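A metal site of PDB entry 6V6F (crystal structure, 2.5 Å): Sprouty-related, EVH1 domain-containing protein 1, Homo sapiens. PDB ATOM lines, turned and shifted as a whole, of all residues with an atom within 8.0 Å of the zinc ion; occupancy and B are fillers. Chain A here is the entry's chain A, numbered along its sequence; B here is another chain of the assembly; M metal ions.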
ATOM      1  N   VAL A  35      19.015  14.927 -24.196  1.00  0.00           N
ATOM      2  CA  VAL A  35      18.816  14.715 -22.768  1.00  0.00           C
ATOM      3  C   VAL A  35      18.548  16.080 -22.147  1.00  0.00           C
ATOM      4  O   VAL A  35      19.363  17.009 -22.295  1.00  0.00           O
ATOM      5  CB  VAL A  35      20.022  14.023 -22.098  1.00  0.00           C
ATOM      6  CG1 VAL A  35      20.116  12.575 -22.570  1.00  0.00           C
ATOM      7  CG2 VAL A  35      21.314  14.749 -22.400  1.00  0.00           C
ATOM      8  N   PRO A  36      17.419  16.275 -21.478  1.00  0.00           N
ATOM      9  CA  PRO A  36      17.006  17.628 -21.097  1.00  0.00           C
ATOM     10  C   PRO A  36      17.675  18.112 -19.825  1.00  0.00           C
ATOM     11  O   PRO A  36      17.977  17.346 -18.913  1.00  0.00           O
ATOM     12  CB  PRO A  36      15.497  17.480 -20.896  1.00  0.00           C
ATOM     13  CG  PRO A  36      15.336  16.065 -20.441  1.00  0.00           C
ATOM     14  CD  PRO A  36      16.383  15.267 -21.167  1.00  0.00           C
ATOM     15  N   HIS A  37      17.912  19.424 -19.786  1.00  0.00           N
ATOM     16  CA  HIS A  37      18.276  20.092 -18.549  1.00  0.00           C
ATOM     17  C   HIS A  37      17.014  20.267 -17.725  1.00  0.00           C
ATOM     18  O   HIS A  37      16.075  20.942 -18.160  1.00  0.00           O
ATOM     19  CB  HIS A  37      18.930  21.454 -18.809  1.00  0.00           C
ATOM     20  CG  HIS A  37      19.964  21.439 -19.900  1.00  0.00           C
ATOM     21  ND1 HIS A  37      20.399  22.588 -20.519  1.00  0.00           N
ATOM     22  CD2 HIS A  37      20.654  20.424 -20.470  1.00  0.00           C
ATOM     23  CE1 HIS A  37      21.304  22.283 -21.427  1.00  0.00           C
ATOM     24  NE2 HIS A  37      21.483  20.978 -21.423  1.00  0.00           N
ATOM     25  N   GLN A  38      16.972  19.688 -16.534  1.00  0.00           N
ATOM     26  CA  GLN A  38      15.755  19.855 -15.689  1.00  0.00           C
ATOM     27  C   GLN A  38      14.537  19.222 -16.363  1.00  0.00           C
ATOM     28  O   GLN A  38      14.546  18.004 -16.579  1.00  0.00           O
ATOM     29  CB  GLN A  38      15.509  21.334 -15.431  1.00  0.00           C
ATOM     30  CG  GLN A  38      16.625  22.004 -14.638  1.00  0.00           C
ATOM     31  CD  GLN A  38      16.968  21.279 -13.369  1.00  0.00           C
ATOM     32  OE1 GLN A  38      16.439  20.216 -13.072  1.00  0.00           O
ATOM     33  NE2 GLN A  38      17.880  21.858 -12.594  1.00  0.00           N
ATOM     34  N   GLU A  39      13.495  20.021 -16.627  1.00  0.00           N
ATOM     35  CA  GLU A  39      12.212  19.567 -17.213  1.00  0.00           C
ATOM     36  C   GLU A  39      12.435  18.954 -18.600  1.00  0.00           C
ATOM     37  O   GLU A  39      13.163  19.553 -19.399  1.00  0.00           O
ATOM     38  CB  GLU A  39      11.258  20.758 -17.269  1.00  0.00           C
ATOM     39  CG  GLU A  39      11.867  21.970 -17.960  1.00  0.00           C
ATOM     40  CD  GLU A  39      12.624  22.916 -17.057  1.00  0.00           C
ATOM     41  OE1 GLU A  39      13.566  23.576 -17.551  1.00  0.00           O
ATOM     42  OE2 GLU A  39      12.257  23.015 -15.868  1.00  0.00           O
ATOM     43  N   GLY A  42      12.097  20.914 -22.203  1.00  0.00           N
ATOM     44  CA  GLY A  42      12.807  22.171 -22.098  1.00  0.00           C
ATOM     45  C   GLY A  42      14.173  22.114 -22.756  1.00  0.00           C
ATOM     46  O   GLY A  42      14.399  21.304 -23.655  1.00  0.00           O
ATOM     47  N   CYS A  43      15.092  22.984 -22.326  1.00  0.00           N
ATOM     48  CA  CYS A  43      16.435  23.006 -22.888  1.00  0.00           C
ATOM     49  C   CYS A  43      17.145  21.682 -22.642  1.00  0.00           C
ATOM     50  O   CYS A  43      16.889  20.981 -21.658  1.00  0.00           O
ATOM     51  CB  CYS A  43      17.236  24.162 -22.290  1.00  0.00           C
ATOM     52  SG  CYS A  43      17.153  24.253 -20.487  1.00  0.00           S
ATOM     53  N   ALA A  44      18.058  21.338 -23.559  1.00  0.00           N
ATOM     54  CA  ALA A  44      18.665  20.014 -23.553  1.00  0.00           C
ATOM     55  C   ALA A  44      20.041  20.061 -24.201  1.00  0.00           C
ATOM     56  O   ALA A  44      20.418  21.054 -24.837  1.00  0.00           O
ATOM     57  CB  ALA A  44      17.774  18.991 -24.271  1.00  0.00           C
ATOM     58  N   ASP A  45      20.796  18.981 -24.023  1.00  0.00           N
ATOM     59  CA  ASP A  45      22.006  18.704 -24.781  1.00  0.00           C
ATOM     60  C   ASP A  45      21.701  17.650 -25.836  1.00  0.00           C
ATOM     61  O   ASP A  45      20.854  16.786 -25.636  1.00  0.00           O
ATOM     62  CB  ASP A  45      23.134  18.226 -23.869  1.00  0.00           C
ATOM     63  CG  ASP A  45      23.562  19.269 -22.864  1.00  0.00           C
ATOM     64  OD1 ASP A  45      23.532  20.471 -23.197  1.00  0.00           O
ATOM     65  OD2 ASP A  45      23.939  18.880 -21.732  1.00  0.00           O
ATOM     66  N   ILE A 111      18.506  23.411 -30.283  1.00  0.00           N
ATOM     67  CA  ILE A 111      19.530  23.569 -29.239  1.00  0.00           C
ATOM     68  C   ILE A 111      19.212  24.773 -28.355  1.00  0.00           C
ATOM     69  O   ILE A 111      19.209  24.662 -27.118  1.00  0.00           O
ATOM     70  CB  ILE A 111      20.924  23.699 -29.879  1.00  0.00           C
ATOM     71  CG1 ILE A 111      21.394  22.336 -30.394  1.00  0.00           C
ATOM     72  CG2 ILE A 111      21.921  24.270 -28.896  1.00  0.00           C
ATOM     73  CD1 ILE A 111      22.811  22.333 -30.944  1.00  0.00           C
ATOM     74  N   SER A 112      18.936  25.922 -28.963  1.00  0.00           N
ATOM     75  CA  SER A 112      18.607  27.159 -28.240  1.00  0.00           C
ATOM     76  C   SER A 112      19.710  27.584 -27.267  1.00  0.00           C
ATOM     77  O   SER A 112      20.806  27.028 -27.257  1.00  0.00           O
ATOM     78  CB  SER A 112      17.283  27.013 -27.477  1.00  0.00           C
ATOM     79  OG  SER A 112      17.434  26.176 -26.337  1.00  0.00           O
ATOM     80  N   ASN B 178      23.697  15.255 -16.741  1.00  0.00           N
ATOM     81  CA  ASN B 178      23.920  16.617 -16.266  1.00  0.00           C
ATOM     82  C   ASN B 178      24.873  16.650 -15.072  1.00  0.00           C
ATOM     83  O   ASN B 178      24.733  17.478 -14.161  1.00  0.00           O
ATOM     84  CB  ASN B 178      22.592  17.295 -15.914  1.00  0.00           C
ATOM     85  CG  ASN B 178      21.793  17.674 -17.137  1.00  0.00           C
ATOM     86  OD1 ASN B 178      21.974  18.764 -17.695  1.00  0.00           O
ATOM     87  ND2 ASN B 178      20.910  16.786 -17.571  1.00  0.00           N
ATOM     88  N   HIS B 230      21.290  26.539 -12.821  1.00  0.00           N
ATOM     89  CA  HIS B 230      20.235  26.268 -13.798  1.00  0.00           C
ATOM     90  C   HIS B 230      18.883  26.153 -13.089  1.00  0.00           C
ATOM     91  O   HIS B 230      18.176  25.151 -13.184  1.00  0.00           O
ATOM     92  CB  HIS B 230      20.541  25.006 -14.620  1.00  0.00           C
ATOM     93  CG  HIS B 230      19.729  24.897 -15.862  1.00  0.00           C
ATOM     94  ND1 HIS B 230      18.379  24.600 -15.847  1.00  0.00           N
ATOM     95  CD2 HIS B 230      20.065  25.050 -17.168  1.00  0.00           C
ATOM     96  CE1 HIS B 230      17.926  24.580 -17.089  1.00  0.00           C
ATOM     97  NE2 HIS B 230      18.925  24.841 -17.903  1.00  0.00           N
ATOM     98  N   LYS B 247      17.021  32.907 -17.029  1.00  0.00           N
ATOM     99  CA  LYS B 247      16.690  31.774 -17.890  1.00  0.00           C
ATOM    100  C   LYS B 247      17.409  31.871 -19.236  1.00  0.00           C
ATOM    101  O   LYS B 247      17.756  30.836 -19.818  1.00  0.00           O
ATOM    102  CB  LYS B 247      15.179  31.701 -18.088  1.00  0.00           C
ATOM    103  CG  LYS B 247      14.710  30.520 -18.936  1.00  0.00           C
ATOM    104  CD  LYS B 247      13.221  30.283 -18.781  1.00  0.00           C
ATOM    105  CE  LYS B 247      12.736  29.115 -19.637  1.00  0.00           C
ATOM    106  NZ  LYS B 247      12.721  29.452 -21.087  1.00  0.00           N
ATOM    107  N   ASN B 249      20.373  32.880 -19.752  1.00  0.00           N
ATOM    108  CA  ASN B 249      21.816  32.675 -19.589  1.00  0.00           C
ATOM    109  C   ASN B 249      22.155  31.290 -19.037  1.00  0.00           C
ATOM    110  O   ASN B 249      23.317  31.042 -18.719  1.00  0.00           O
ATOM    111  CB  ASN B 249      22.410  33.761 -18.687  1.00  0.00           C
ATOM    112  CG  ASN B 249      22.479  35.107 -19.373  1.00  0.00           C
ATOM    113  OD1 ASN B 249      23.264  35.305 -20.302  1.00  0.00           O
ATOM    114  ND2 ASN B 249      21.676  36.053 -18.901  1.00  0.00           N
ATOM    115  N   PHE B 250      21.172  30.396 -18.925  1.00  0.00           N
ATOM    116  CA  PHE B 250      21.432  29.052 -18.424  1.00  0.00           C
ATOM    117  C   PHE B 250      22.484  28.342 -19.261  1.00  0.00           C
ATOM    118  O   PHE B 250      23.557  27.968 -18.767  1.00  0.00           O
ATOM    119  CB  PHE B 250      20.136  28.238 -18.409  1.00  0.00           C
ATOM    120  CG  PHE B 250      19.263  28.502 -17.214  1.00  0.00           C
ATOM    121  CD1 PHE B 250      19.784  29.095 -16.080  1.00  0.00           C
ATOM    122  CD2 PHE B 250      17.927  28.141 -17.227  1.00  0.00           C
ATOM    123  CE1 PHE B 250      18.987  29.334 -14.980  1.00  0.00           C
ATOM    124  CE2 PHE B 250      17.123  28.373 -16.137  1.00  0.00           C
ATOM    125  CZ  PHE B 250      17.650  28.969 -15.010  1.00  0.00           C
ATOM    126  N   ASP B 251      22.198  28.150 -20.554  1.00  0.00           N
ATOM    127  CA  ASP B 251      23.044  27.308 -21.388  1.00  0.00           C
ATOM    128  C   ASP B 251      24.351  27.993 -21.778  1.00  0.00           C
ATOM    129  O   ASP B 251      25.298  27.298 -22.173  1.00  0.00           O
ATOM    130  CB  ASP B 251      22.275  26.880 -22.640  1.00  0.00           C
ATOM    131  CG  ASP B 251      21.062  26.056 -22.309  1.00  0.00           C
ATOM    132  OD1 ASP B 251      20.901  25.679 -21.138  1.00  0.00           O
ATOM    133  OD2 ASP B 251      20.256  25.793 -23.222  1.00  0.00           O
ATOM    134  N   ALA B 252      24.431  29.322 -21.674  1.00  0.00           N
ATOM    135  CA  ALA B 252      25.706  29.991 -21.890  1.00  0.00           C
ATOM    136  C   ALA B 252      26.698  29.647 -20.777  1.00  0.00           C
ATOM    137  O   ALA B 252      27.912  29.646 -21.018  1.00  0.00           O
ATOM    138  CB  ALA B 252      25.501  31.496 -21.988  1.00  0.00           C
ATOM    139  N   ARG B 254      26.652  26.643 -19.135  1.00  0.00           N
ATOM    140  CA  ARG B 254      27.021  25.249 -19.335  1.00  0.00           C
ATOM    141  C   ARG B 254      28.108  25.104 -20.394  1.00  0.00           C
ATOM    142  O   ARG B 254      29.019  24.282 -20.238  1.00  0.00           O
ATOM    143  CB  ARG B 254      25.785  24.423 -19.717  1.00  0.00           C
ATOM    144  CG  ARG B 254      24.784  24.241 -18.593  1.00  0.00           C
ATOM    145  CD  ARG B 254      23.581  23.438 -19.061  1.00  0.00           C
ATOM    146  NE  ARG B 254      23.980  22.176 -19.665  1.00  0.00           N
ATOM    147  CZ  ARG B 254      24.048  21.024 -19.002  1.00  0.00           C
ATOM    148  NH1 ARG B 254      24.423  19.913 -19.633  1.00  0.00           N
ATOM    149  NH2 ARG B 254      23.755  20.975 -17.712  1.00  0.00           N
HETATM  150 ZN    ZN M   1      19.514  24.484 -20.183  1.00  0.00          ZN
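O of His 230 of chain B lies within hydrogen-bond range of NE2 of Gln 38 (3.4 Å). NE2 of His 37 sits close to NE of Arg 254 of chain B. A ring nitrogen (NE2) of His 37 lies within hydrogen-bond range of the side-chain carboxylate (OD1) of Asp 45, 2.8 Å away.
Of the 19 residues printed, 4 come within 4 Å of the zinc ion.
The zinc ion is bound by the side-chain carboxylate of Asp 251 of chain B (2.1 Å), a ring nitrogen (ND1) of His 37 (2.1 Å), a ring nitrogen (NE2) of His 230 of chain B (2.4 Å) and the side-chain sulfur of Cys 43 (2.4 Å).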
